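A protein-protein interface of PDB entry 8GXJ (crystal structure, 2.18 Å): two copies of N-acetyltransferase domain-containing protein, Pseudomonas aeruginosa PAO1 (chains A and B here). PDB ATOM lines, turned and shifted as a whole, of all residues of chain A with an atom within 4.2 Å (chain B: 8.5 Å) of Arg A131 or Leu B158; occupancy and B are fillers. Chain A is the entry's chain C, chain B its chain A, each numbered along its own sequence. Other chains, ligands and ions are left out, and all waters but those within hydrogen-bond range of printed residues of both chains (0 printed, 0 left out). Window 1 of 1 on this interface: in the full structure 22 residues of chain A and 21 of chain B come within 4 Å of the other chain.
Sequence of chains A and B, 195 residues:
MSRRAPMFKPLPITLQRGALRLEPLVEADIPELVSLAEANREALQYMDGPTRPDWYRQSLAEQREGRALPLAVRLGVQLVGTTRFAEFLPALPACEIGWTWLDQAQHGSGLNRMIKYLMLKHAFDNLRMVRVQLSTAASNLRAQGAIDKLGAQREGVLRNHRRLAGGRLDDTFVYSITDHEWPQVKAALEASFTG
The backbone carbonyl oxygen of Glu A155 sits at hydrogen-bond distance from the backbone NH of Val B157.
The guanidinium group (NH2) of Arg A131 sits at hydrogen-bond distance from the backbone carbonyl oxygen (O) of Arg B159, 2.9 Å away.
NE of Arg B159 is in salt-bridge range of OE2 of Glu A155.
NH2 of Arg B159 sits at hydrogen-bond distance from OG of Ser A176 (3.4 Å).
O of Val A130 is in hydrogen-bond range of ND2 of Asn B160, at 3.1 Å.
N of Asn B160 is in hydrogen-bond range of OD1 of Asp B171, at 3.1 Å.
A ring nitrogen (ND1) of His B161 sits at hydrogen-bond distance from the side-chain hydroxyl (OG1) of Thr B172 (2.8 Å).
NH1 of Arg A131 sits at hydrogen-bond distance from OE1 of Gln A133 (3.0 Å).
The guanidinium group (NH2) of Arg A131 lies within salt-bridge range of the side-chain carboxylate (OE1) of Glu A155 (2.6 Å).
The guanidinium group (NH2) of Arg A131 lies close to the side-chain hydroxyl (OG) of Ser A176, at 3.4 Å.
OG of Ser A176 lies within hydrogen-bond range of OE2 of Glu A155 (2.6 Å).
Among the printed residues, merely in contact across the chains: Glu A155 with Gly B156, Glu A155 with Leu B158, Arg A131 with Asn B160, Arg A131 with Leu B158, Arg A131 with His B161 and Val A130 with Leu B169.
Arg A131 touches just these residues of chain B: Leu B158 (3.7 Å), Arg B159 (2.9 Å), Asn B160 (3.6 Å) and His B161 (3.7 Å).
Of the printed residues of chain B, Glu A155 touches Gly B156, Val B157, Leu B158 and Arg B159.
Printed residues of chain A within 4 Å of His B161: Arg A131.
The nearest printed residue of chain A that does not touch Gly B156 is Val A174 (7.5 Å).
Of the 13 printed residues of chain A, 4 touch a printed residue of chain B.
Of the 23 printed residues of chain B, 7 touch a printed residue of chain A.
Printed residues of chain B that touch a printed residue of chain A: Gly B156, Val B157, Leu B158, Arg B159, Asn B160, His B161 and Leu B169.
Hydrophobic or aromatic side chains of chain B that line the printed part of chain A: Leu B158, His B161 and Leu B169.
Among the printed residues, Asp or Glu carboxylates within 4 Å of a Lys or Arg side-chain nitrogen of the other chain: Glu A155 with Arg B159.
Positions printed for both chains: 133, 155 and 174.
Of the 11 pairs that touch across the chains among the printed residues, none has its exchanged pair printed and touching as well.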
ATOM      1  N   PRO A  93      25.978  18.115  28.530  1.00  0.00           N
ATOM      2  CA  PRO A  93      26.413  16.737  28.276  1.00  0.00           C
ATOM      3  C   PRO A  93      25.832  16.249  26.955  1.00  0.00           C
ATOM      4  O   PRO A  93      24.802  16.752  26.481  1.00  0.00           O
ATOM      5  CB  PRO A  93      25.842  15.960  29.469  1.00  0.00           C
ATOM      6  CG  PRO A  93      24.566  16.711  29.799  1.00  0.00           C
ATOM      7  CD  PRO A  93      24.764  18.157  29.370  1.00  0.00           C
ATOM      8  N   ALA A  94      26.500  15.278  26.350  1.00  0.00           N
ATOM      9  CA  ALA A  94      26.042  14.727  25.085  1.00  0.00           C
ATOM     10  C   ALA A  94      26.464  13.269  25.014  1.00  0.00           C
ATOM     11  O   ALA A  94      27.340  12.820  25.763  1.00  0.00           O
ATOM     12  CB  ALA A  94      26.609  15.498  23.893  1.00  0.00           C
ATOM     13  N   CYS A  95      25.844  12.531  24.101  1.00  0.00           N
ATOM     14  CA  CYS A  95      26.267  11.152  23.899  1.00  0.00           C
ATOM     15  C   CYS A  95      25.809  10.690  22.528  1.00  0.00           C
ATOM     16  O   CYS A  95      25.121  11.410  21.795  1.00  0.00           O
ATOM     17  CB  CYS A  95      25.712  10.235  24.997  1.00  0.00           C
ATOM     18  SG  CYS A  95      23.921   9.997  24.854  1.00  0.00           S
ATOM     19  N   PHE A 124      17.540  12.971  27.143  1.00  0.00           N
ATOM     20  CA  PHE A 124      17.089  14.356  27.157  1.00  0.00           C
ATOM     21  C   PHE A 124      16.295  14.696  28.402  1.00  0.00           C
ATOM     22  O   PHE A 124      16.514  15.751  28.995  1.00  0.00           O
ATOM     23  CB  PHE A 124      16.228  14.643  25.931  1.00  0.00           C
ATOM     24  CG  PHE A 124      17.004  14.764  24.677  1.00  0.00           C
ATOM     25  CD1 PHE A 124      17.971  15.734  24.551  1.00  0.00           C
ATOM     26  CD2 PHE A 124      16.765  13.905  23.614  1.00  0.00           C
ATOM     27  CE1 PHE A 124      18.705  15.845  23.372  1.00  0.00           C
ATOM     28  CE2 PHE A 124      17.474  14.021  22.438  1.00  0.00           C
ATOM     29  CZ  PHE A 124      18.452  14.982  22.314  1.00  0.00           C
ATOM     30  N   MET A 129      20.442  16.090  28.185  1.00  0.00           N
ATOM     31  CA  MET A 129      21.509  16.299  27.234  1.00  0.00           C
ATOM     32  C   MET A 129      21.121  17.362  26.224  1.00  0.00           C
ATOM     33  O   MET A 129      19.948  17.597  25.948  1.00  0.00           O
ATOM     34  CB  MET A 129      21.866  14.987  26.568  1.00  0.00           C
ATOM     35  CG  MET A 129      22.628  14.213  27.565  1.00  0.00           C
ATOM     36  SD  MET A 129      23.054  12.650  26.914  1.00  0.00           S
ATOM     37  CE  MET A 129      24.231  12.138  28.126  1.00  0.00           C
ATOM     38  N   VAL A 130      22.135  18.039  25.707  1.00  0.00           N
ATOM     39  CA  VAL A 130      21.908  19.053  24.690  1.00  0.00           C
ATOM     40  C   VAL A 130      22.038  18.469  23.293  1.00  0.00           C
ATOM     41  O   VAL A 130      21.582  19.087  22.317  1.00  0.00           O
ATOM     42  CB  VAL A 130      22.874  20.214  24.975  1.00  0.00           C
ATOM     43  CG1 VAL A 130      22.677  20.684  26.430  1.00  0.00           C
ATOM     44  CG2 VAL A 130      24.328  19.774  24.760  1.00  0.00           C
ATOM     45  N   ARG A 131      22.601  17.268  23.172  1.00  0.00           N
ATOM     46  CA  ARG A 131      22.874  16.652  21.880  1.00  0.00           C
ATOM     47  C   ARG A 131      22.850  15.143  22.052  1.00  0.00           C
ATOM     48  O   ARG A 131      23.542  14.615  22.924  1.00  0.00           O
ATOM     49  CB  ARG A 131      24.237  17.115  21.359  1.00  0.00           C
ATOM     50  CG  ARG A 131      24.756  16.346  20.192  1.00  0.00           C
ATOM     51  CD  ARG A 131      26.225  16.692  19.917  1.00  0.00           C
ATOM     52  NE  ARG A 131      26.695  15.860  18.826  1.00  0.00           N
ATOM     53  CZ  ARG A 131      26.446  16.107  17.546  1.00  0.00           C
ATOM     54  NH1 ARG A 131      26.888  15.259  16.607  1.00  0.00           N
ATOM     55  NH2 ARG A 131      25.767  17.205  17.205  1.00  0.00           N
ATOM     56  N   VAL A 132      22.041  14.448  21.256  1.00  0.00           N
ATOM     57  CA  VAL A 132      22.205  13.012  21.097  1.00  0.00           C
ATOM     58  C   VAL A 132      22.634  12.749  19.666  1.00  0.00           C
ATOM     59  O   VAL A 132      21.969  13.180  18.715  1.00  0.00           O
ATOM     60  CB  VAL A 132      20.944  12.212  21.455  1.00  0.00           C
ATOM     61  CG1 VAL A 132      21.160  10.730  21.061  1.00  0.00           C
ATOM     62  CG2 VAL A 132      20.670  12.337  22.968  1.00  0.00           C
ATOM     63  N   GLN A 133      23.756  12.070  19.517  1.00  0.00           N
ATOM     64  CA  GLN A 133      24.294  11.733  18.217  1.00  0.00           C
ATOM     65  C   GLN A 133      23.873  10.326  17.792  1.00  0.00           C
ATOM     66  O   GLN A 133      23.774   9.416  18.617  1.00  0.00           O
ATOM     67  CB  GLN A 133      25.806  11.847  18.266  1.00  0.00           C
ATOM     68  CG  GLN A 133      26.476  11.372  17.053  1.00  0.00           C
ATOM     69  CD  GLN A 133      27.951  11.594  17.145  1.00  0.00           C
ATOM     70  OE1 GLN A 133      28.402  12.739  17.164  1.00  0.00           O
ATOM     71  NE2 GLN A 133      28.720  10.507  17.188  1.00  0.00           N
ATOM     72  N   GLU A 155      24.212  15.775  10.049  1.00  0.00           N
ATOM     73  CA  GLU A 155      25.121  16.852  10.405  1.00  0.00           C
ATOM     74  C   GLU A 155      26.451  16.786   9.687  1.00  0.00           C
ATOM     75  O   GLU A 155      27.098  17.821   9.544  1.00  0.00           O
ATOM     76  CB  GLU A 155      25.396  16.844  11.912  1.00  0.00           C
ATOM     77  CG  GLU A 155      24.271  17.353  12.767  1.00  0.00           C
ATOM     78  CD  GLU A 155      24.706  17.499  14.230  1.00  0.00           C
ATOM     79  OE1 GLU A 155      25.580  16.709  14.676  1.00  0.00           O
ATOM     80  OE2 GLU A 155      24.178  18.393  14.927  1.00  0.00           O
ATOM     81  N   VAL A 174      26.862  11.205  10.114  1.00  0.00           N
ATOM     82  CA  VAL A 174      26.630  11.581  11.501  1.00  0.00           C
ATOM     83  C   VAL A 174      25.373  12.435  11.555  1.00  0.00           C
ATOM     84  O   VAL A 174      25.218  13.376  10.768  1.00  0.00           O
ATOM     85  CB  VAL A 174      27.834  12.337  12.087  1.00  0.00           C
ATOM     86  CG1 VAL A 174      27.616  12.645  13.575  1.00  0.00           C
ATOM     87  CG2 VAL A 174      29.090  11.531  11.894  1.00  0.00           C
ATOM     88  N   SER A 176      22.254  14.194  14.427  1.00  0.00           N
ATOM     89  CA  SER A 176      22.013  14.511  15.824  1.00  0.00           C
ATOM     90  C   SER A 176      20.593  15.005  16.043  1.00  0.00           C
ATOM     91  O   SER A 176      19.867  15.356  15.108  1.00  0.00           O
ATOM     92  CB  SER A 176      23.022  15.538  16.360  1.00  0.00           C
ATOM     93  OG  SER A 176      22.552  16.869  16.192  1.00  0.00           O
ATOM     94  N   ILE A 177      20.209  14.980  17.315  1.00  0.00           N
ATOM     95  CA  ILE A 177      19.016  15.628  17.836  1.00  0.00           C
ATOM     96  C   ILE A 177      19.474  16.559  18.944  1.00  0.00           C
ATOM     97  O   ILE A 177      20.186  16.132  19.859  1.00  0.00           O
ATOM     98  CB  ILE A 177      17.993  14.604  18.368  1.00  0.00           C
ATOM     99  CG1 ILE A 177      17.656  13.572  17.293  1.00  0.00           C
ATOM    100  CG2 ILE A 177      16.731  15.306  18.913  1.00  0.00           C
ATOM    101  CD1 ILE A 177      16.968  12.305  17.854  1.00  0.00           C
ATOM    102  N   GLU B  96      42.944  12.552  15.179  1.00  0.00           N
ATOM    103  CA  GLU B  96      42.623  13.960  15.119  1.00  0.00           C
ATOM    104  C   GLU B  96      43.851  14.743  15.564  1.00  0.00           C
ATOM    105  O   GLU B  96      44.569  14.333  16.485  1.00  0.00           O
ATOM    106  CB  GLU B  96      41.397  14.280  16.002  1.00  0.00           C
ATOM    107  CG  GLU B  96      41.152  15.771  16.100  1.00  0.00           C
ATOM    108  CD  GLU B  96      39.732  16.156  16.512  1.00  0.00           C
ATOM    109  OE1 GLU B  96      38.877  15.267  16.717  1.00  0.00           O
ATOM    110  OE2 GLU B  96      39.478  17.371  16.618  1.00  0.00           O
ATOM    111  N   GLN B 133      41.429  13.992  11.150  1.00  0.00           N
ATOM    112  CA  GLN B 133      40.366  14.942  11.384  1.00  0.00           C
ATOM    113  C   GLN B 133      40.944  16.224  11.973  1.00  0.00           C
ATOM    114  O   GLN B 133      41.893  16.187  12.763  1.00  0.00           O
ATOM    115  CB  GLN B 133      39.344  14.329  12.330  1.00  0.00           C
ATOM    116  CG  GLN B 133      38.133  15.185  12.559  1.00  0.00           C
ATOM    117  CD  GLN B 133      37.108  14.464  13.385  1.00  0.00           C
ATOM    118  OE1 GLN B 133      36.540  13.464  12.942  1.00  0.00           O
ATOM    119  NE2 GLN B 133      36.860  14.963  14.604  1.00  0.00           N
ATOM    120  N   SER B 135      39.117  19.849  13.682  1.00  0.00           N
ATOM    121  CA  SER B 135      37.852  20.462  14.049  1.00  0.00           C
ATOM    122  C   SER B 135      38.133  21.730  14.832  1.00  0.00           C
ATOM    123  O   SER B 135      39.233  21.941  15.338  1.00  0.00           O
ATOM    124  CB  SER B 135      36.970  19.503  14.856  1.00  0.00           C
ATOM    125  OG  SER B 135      37.539  19.213  16.111  1.00  0.00           O
ATOM    126  N   THR B 136      37.122  22.586  14.905  1.00  0.00           N
ATOM    127  CA  THR B 136      37.254  23.828  15.640  1.00  0.00           C
ATOM    128  C   THR B 136      35.859  24.343  15.962  1.00  0.00           C
ATOM    129  O   THR B 136      34.862  23.862  15.422  1.00  0.00           O
ATOM    130  CB  THR B 136      38.065  24.845  14.833  1.00  0.00           C
ATOM    131  OG1 THR B 136      38.497  25.882  15.713  1.00  0.00           O
ATOM    132  CG2 THR B 136      37.208  25.443  13.684  1.00  0.00           C
ATOM    133  N   ALA B 137      35.801  25.335  16.850  1.00  0.00           N
ATOM    134  CA  ALA B 137      34.521  25.903  17.252  1.00  0.00           C
ATOM    135  C   ALA B 137      33.869  26.607  16.067  1.00  0.00           C
ATOM    136  O   ALA B 137      34.544  27.211  15.225  1.00  0.00           O
ATOM    137  CB  ALA B 137      34.716  26.886  18.413  1.00  0.00           C
ATOM    138  N   ALA B 138      32.551  26.520  15.990  1.00  0.00           N
ATOM    139  CA  ALA B 138      31.858  27.230  14.921  1.00  0.00           C
ATOM    140  C   ALA B 138      32.131  28.731  14.980  1.00  0.00           C
ATOM    141  O   ALA B 138      32.153  29.398  13.941  1.00  0.00           O
ATOM    142  CB  ALA B 138      30.352  26.940  14.990  1.00  0.00           C
ATOM    143  N   ARG B 154      35.754  20.616   4.692  1.00  0.00           N
ATOM    144  CA  ARG B 154      34.742  20.567   5.737  1.00  0.00           C
ATOM    145  C   ARG B 154      33.850  19.367   5.491  1.00  0.00           C
ATOM    146  O   ARG B 154      33.500  19.045   4.351  1.00  0.00           O
ATOM    147  CB  ARG B 154      33.908  21.845   5.805  1.00  0.00           C
ATOM    148  CG  ARG B 154      33.284  22.103   7.214  1.00  0.00           C
ATOM    149  CD  ARG B 154      32.407  23.311   7.182  1.00  0.00           C
ATOM    150  NE  ARG B 154      31.610  23.189   5.997  1.00  0.00           N
ATOM    151  CZ  ARG B 154      31.742  24.005   4.964  1.00  0.00           C
ATOM    152  NH1 ARG B 154      32.610  25.010   4.989  1.00  0.00           N
ATOM    153  NH2 ARG B 154      31.012  23.789   3.912  1.00  0.00           N
ATOM    154  N   GLU B 155      33.526  18.668   6.564  1.00  0.00           N
ATOM    155  CA  GLU B 155      32.707  17.480   6.457  1.00  0.00           C
ATOM    156  C   GLU B 155      31.376  17.612   7.154  1.00  0.00           C
ATOM    157  O   GLU B 155      30.451  16.872   6.820  1.00  0.00           O
ATOM    158  CB  GLU B 155      33.454  16.268   7.024  1.00  0.00           C
ATOM    159  CG  GLU B 155      34.621  15.826   6.164  1.00  0.00           C
ATOM    160  CD  GLU B 155      35.343  14.631   6.766  1.00  0.00           C
ATOM    161  OE1 GLU B 155      35.602  14.638   7.992  1.00  0.00           O
ATOM    162  OE2 GLU B 155      35.649  13.689   6.016  1.00  0.00           O
ATOM    163  N   GLY B 156      31.247  18.523   8.103  1.00  0.00           N
ATOM    164  CA  GLY B 156      29.955  18.747   8.700  1.00  0.00           C
ATOM    165  C   GLY B 156      30.049  19.769   9.808  1.00  0.00           C
ATOM    166  O   GLY B 156      31.107  20.342  10.068  1.00  0.00           O
ATOM    167  N   VAL B 157      28.901  19.998  10.443  1.00  0.00           N
ATOM    168  CA  VAL B 157      28.787  20.937  11.550  1.00  0.00           C
ATOM    169  C   VAL B 157      27.994  20.223  12.636  1.00  0.00           C
ATOM    170  O   VAL B 157      26.814  19.906  12.442  1.00  0.00           O
ATOM    171  CB  VAL B 157      28.098  22.244  11.136  1.00  0.00           C
ATOM    172  CG1 VAL B 157      27.992  23.205  12.322  1.00  0.00           C
ATOM    173  CG2 VAL B 157      28.857  22.883   9.981  1.00  0.00           C
ATOM    174  N   LEU B 158      28.643  19.944  13.758  1.00  0.00           N
ATOM    175  CA  LEU B 158      28.014  19.240  14.865  1.00  0.00           C
ATOM    176  C   LEU B 158      27.408  20.258  15.825  1.00  0.00           C
ATOM    177  O   LEU B 158      28.134  21.063  16.419  1.00  0.00           O
ATOM    178  CB  LEU B 158      29.038  18.354  15.573  1.00  0.00           C
ATOM    179  CG  LEU B 158      29.792  17.390  14.643  1.00  0.00           C
ATOM    180  CD1 LEU B 158      30.751  16.456  15.398  1.00  0.00           C
ATOM    181  CD2 LEU B 158      28.830  16.566  13.779  1.00  0.00           C
ATOM    182  N   ARG B 159      26.088  20.218  15.977  1.00  0.00           N
ATOM    183  CA  ARG B 159      25.406  21.182  16.833  1.00  0.00           C
ATOM    184  C   ARG B 159      25.556  20.828  18.309  1.00  0.00           C
ATOM    185  O   ARG B 159      25.606  19.652  18.684  1.00  0.00           O
ATOM    186  CB  ARG B 159      23.929  21.269  16.450  1.00  0.00           C
ATOM    187  CG  ARG B 159      23.774  21.663  14.987  1.00  0.00           C
ATOM    188  CD  ARG B 159      22.342  21.573  14.529  1.00  0.00           C
ATOM    189  NE  ARG B 159      21.797  20.230  14.710  1.00  0.00           N
ATOM    190  CZ  ARG B 159      20.493  19.975  14.756  1.00  0.00           C
ATOM    191  NH1 ARG B 159      19.627  20.979  14.635  1.00  0.00           N
ATOM    192  NH2 ARG B 159      20.054  18.732  14.937  1.00  0.00           N
ATOM    193  N   ASN B 160      25.656  21.876  19.137  1.00  0.00           N
ATOM    194  CA  ASN B 160      25.698  21.767  20.602  1.00  0.00           C
ATOM    195  C   ASN B 160      26.774  20.790  21.039  1.00  0.00           C
ATOM    196  O   ASN B 160      26.530  19.844  21.787  1.00  0.00           O
ATOM    197  CB  ASN B 160      24.343  21.347  21.174  1.00  0.00           C
ATOM    198  CG  ASN B 160      23.271  22.373  20.949  1.00  0.00           C
ATOM    199  OD1 ASN B 160      23.546  23.477  20.504  1.00  0.00           O
ATOM    200  ND2 ASN B 160      22.036  22.014  21.248  1.00  0.00           N
ATOM    201  N   HIS B 161      27.965  20.996  20.537  1.00  0.00           N
ATOM    202  CA  HIS B 161      28.962  19.963  20.614  1.00  0.00           C
ATOM    203  C   HIS B 161      30.162  20.337  21.459  1.00  0.00           C
ATOM    204  O   HIS B 161      30.990  19.464  21.744  1.00  0.00           O
ATOM    205  CB  HIS B 161      29.398  19.584  19.194  1.00  0.00           C
ATOM    206  CG  HIS B 161      30.355  18.442  19.142  1.00  0.00           C
ATOM    207  ND1 HIS B 161      31.708  18.619  18.951  1.00  0.00           N
ATOM    208  CD2 HIS B 161      30.158  17.110  19.276  1.00  0.00           C
ATOM    209  CE1 HIS B 161      32.301  17.440  18.939  1.00  0.00           C
ATOM    210  NE2 HIS B 161      31.386  16.508  19.138  1.00  0.00           N
ATOM    211  N   ARG B 162      30.267  21.583  21.899  1.00  0.00           N
ATOM    212  CA  ARG B 162      31.400  22.010  22.712  1.00  0.00           C
ATOM    213  C   ARG B 162      30.986  23.219  23.538  1.00  0.00           C
ATOM    214  O   ARG B 162      29.990  23.879  23.243  1.00  0.00           O
ATOM    215  CB  ARG B 162      32.619  22.356  21.846  1.00  0.00           C
ATOM    216  CG  ARG B 162      32.407  23.580  20.953  1.00  0.00           C
ATOM    217  CD  ARG B 162      33.745  24.078  20.403  1.00  0.00           C
ATOM    218  NE  ARG B 162      34.323  23.101  19.479  1.00  0.00           N
ATOM    219  CZ  ARG B 162      35.622  22.851  19.350  1.00  0.00           C
ATOM    220  NH1 ARG B 162      36.509  23.497  20.085  1.00  0.00           N
ATOM    221  NH2 ARG B 162      36.030  21.945  18.474  1.00  0.00           N
ATOM    222  N   ARG B 163      31.768  23.512  24.571  1.00  0.00           N
ATOM    223  CA  ARG B 163      31.572  24.710  25.379  1.00  0.00           C
ATOM    224  C   ARG B 163      32.828  25.565  25.306  1.00  0.00           C
ATOM    225  O   ARG B 163      33.937  25.048  25.437  1.00  0.00           O
ATOM    226  CB  ARG B 163      31.225  24.350  26.832  1.00  0.00           C
ATOM    227  CG  ARG B 163      29.811  23.779  26.959  1.00  0.00           C
ATOM    228  CD  ARG B 163      29.360  23.589  28.387  1.00  0.00           C
ATOM    229  NE  ARG B 163      28.024  23.001  28.409  1.00  0.00           N
ATOM    230  CZ  ARG B 163      26.891  23.684  28.287  1.00  0.00           C
ATOM    231  NH1 ARG B 163      26.903  25.009  28.152  1.00  0.00           N
ATOM    232  NH2 ARG B 163      25.732  23.031  28.307  1.00  0.00           N
ATOM    233  N   LEU B 169      27.568  27.263  24.979  1.00  0.00           N
ATOM    234  CA  LEU B 169      27.467  26.164  24.021  1.00  0.00           C
ATOM    235  C   LEU B 169      27.798  26.648  22.617  1.00  0.00           C
ATOM    236  O   LEU B 169      27.309  27.696  22.186  1.00  0.00           O
ATOM    237  CB  LEU B 169      26.055  25.576  24.033  1.00  0.00           C
ATOM    238  CG  LEU B 169      25.868  24.189  24.635  1.00  0.00           C
ATOM    239  CD1 LEU B 169      24.443  23.709  24.451  1.00  0.00           C
ATOM    240  CD2 LEU B 169      26.831  23.224  24.002  1.00  0.00           C
ATOM    241  N   ASP B 170      28.611  25.875  21.897  1.00  0.00           N
ATOM    242  CA  ASP B 170      28.898  26.171  20.496  1.00  0.00           C
ATOM    243  C   ASP B 170      28.856  24.901  19.651  1.00  0.00           C
ATOM    244  O   ASP B 170      29.018  23.784  20.151  1.00  0.00           O
ATOM    245  CB  ASP B 170      30.268  26.847  20.324  1.00  0.00           C
ATOM    246  CG  ASP B 170      30.415  27.547  18.943  1.00  0.00           C
ATOM    247  OD1 ASP B 170      29.426  27.574  18.165  1.00  0.00           O
ATOM    248  OD2 ASP B 170      31.515  28.069  18.643  1.00  0.00           O
ATOM    249  N   ASP B 171      28.659  25.093  18.354  1.00  0.00           N
ATOM    250  CA  ASP B 171      28.790  24.026  17.378  1.00  0.00           C
ATOM    251  C   ASP B 171      30.261  23.791  17.041  1.00  0.00           C
ATOM    252  O   ASP B 171      31.144  24.573  17.399  1.00  0.00           O
ATOM    253  CB  ASP B 171      28.020  24.360  16.101  1.00  0.00           C
ATOM    254  CG  ASP B 171      26.542  24.683  16.353  1.00  0.00           C
ATOM    255  OD1 ASP B 171      26.011  24.403  17.459  1.00  0.00           O
ATOM    256  OD2 ASP B 171      25.901  25.214  15.417  1.00  0.00           O
ATOM    257  N   THR B 172      30.517  22.693  16.335  1.00  0.00           N
ATOM    258  CA  THR B 172      31.856  22.299  15.927  1.00  0.00           C
ATOM    259  C   THR B 172      31.888  22.136  14.415  1.00  0.00           C
ATOM    260  O   THR B 172      31.063  21.412  13.856  1.00  0.00           O
ATOM    261  CB  THR B 172      32.256  20.980  16.590  1.00  0.00           C
ATOM    262  OG1 THR B 172      32.411  21.182  18.001  1.00  0.00           O
ATOM    263  CG2 THR B 172      33.552  20.451  16.003  1.00  0.00           C
ATOM    264  N   PHE B 173      32.832  22.798  13.752  1.00  0.00           N
ATOM    265  CA  PHE B 173      33.095  22.519  12.346  1.00  0.00           C
ATOM    266  C   PHE B 173      34.094  21.380  12.294  1.00  0.00           C
ATOM    267  O   PHE B 173      35.112  21.428  12.985  1.00  0.00           O
ATOM    268  CB  PHE B 173      33.660  23.740  11.620  1.00  0.00           C
ATOM    269  CG  PHE B 173      32.624  24.767  11.250  1.00  0.00           C
ATOM    270  CD1 PHE B 173      31.496  24.967  12.043  1.00  0.00           C
ATOM    271  CD2 PHE B 173      32.789  25.547  10.124  1.00  0.00           C
ATOM    272  CE1 PHE B 173      30.537  25.919  11.697  1.00  0.00           C
ATOM    273  CE2 PHE B 173      31.831  26.513   9.781  1.00  0.00           C
ATOM    274  CZ  PHE B 173      30.708  26.688  10.570  1.00  0.00           C
ATOM    275  N   VAL B 174      33.802  20.351  11.494  1.00  0.00           N
ATOM    276  CA  VAL B 174      34.671  19.187  11.374  1.00  0.00           C
ATOM    277  C   VAL B 174      35.191  19.102   9.949  1.00  0.00           C
ATOM    278  O   VAL B 174      34.422  19.204   8.987  1.00  0.00           O
ATOM    279  CB  VAL B 174      33.959  17.887  11.784  1.00  0.00           C
ATOM    280  CG1 VAL B 174      33.555  17.981  13.228  1.00  0.00           C
ATOM    281  CG2 VAL B 174      32.740  17.632  10.907  1.00  0.00           C
ATOM    282  N   TYR B 175      36.501  18.931   9.829  1.00  0.00           N
ATOM    283  CA  TYR B 175      37.229  18.848   8.576  1.00  0.00           C
ATOM    284  C   TYR B 175      38.064  17.579   8.600  1.00  0.00           C
ATOM    285  O   TYR B 175      38.393  17.058   9.671  1.00  0.00           O
ATOM    286  CB  TYR B 175      38.190  20.032   8.371  1.00  0.00           C
ATOM    287  CG  TYR B 175      37.604  21.405   8.516  1.00  0.00           C
ATOM    288  CD1 TYR B 175      37.327  21.937   9.775  1.00  0.00           C
ATOM    289  CD2 TYR B 175      37.349  22.190   7.390  1.00  0.00           C
ATOM    290  CE1 TYR B 175      36.797  23.223   9.917  1.00  0.00           C
ATOM    291  CE2 TYR B 175      36.819  23.466   7.517  1.00  0.00           C
ATOM    292  CZ  TYR B 175      36.555  23.976   8.786  1.00  0.00           C
ATOM    293  OH  TYR B 175      36.040  25.227   8.923  1.00  0.00           O
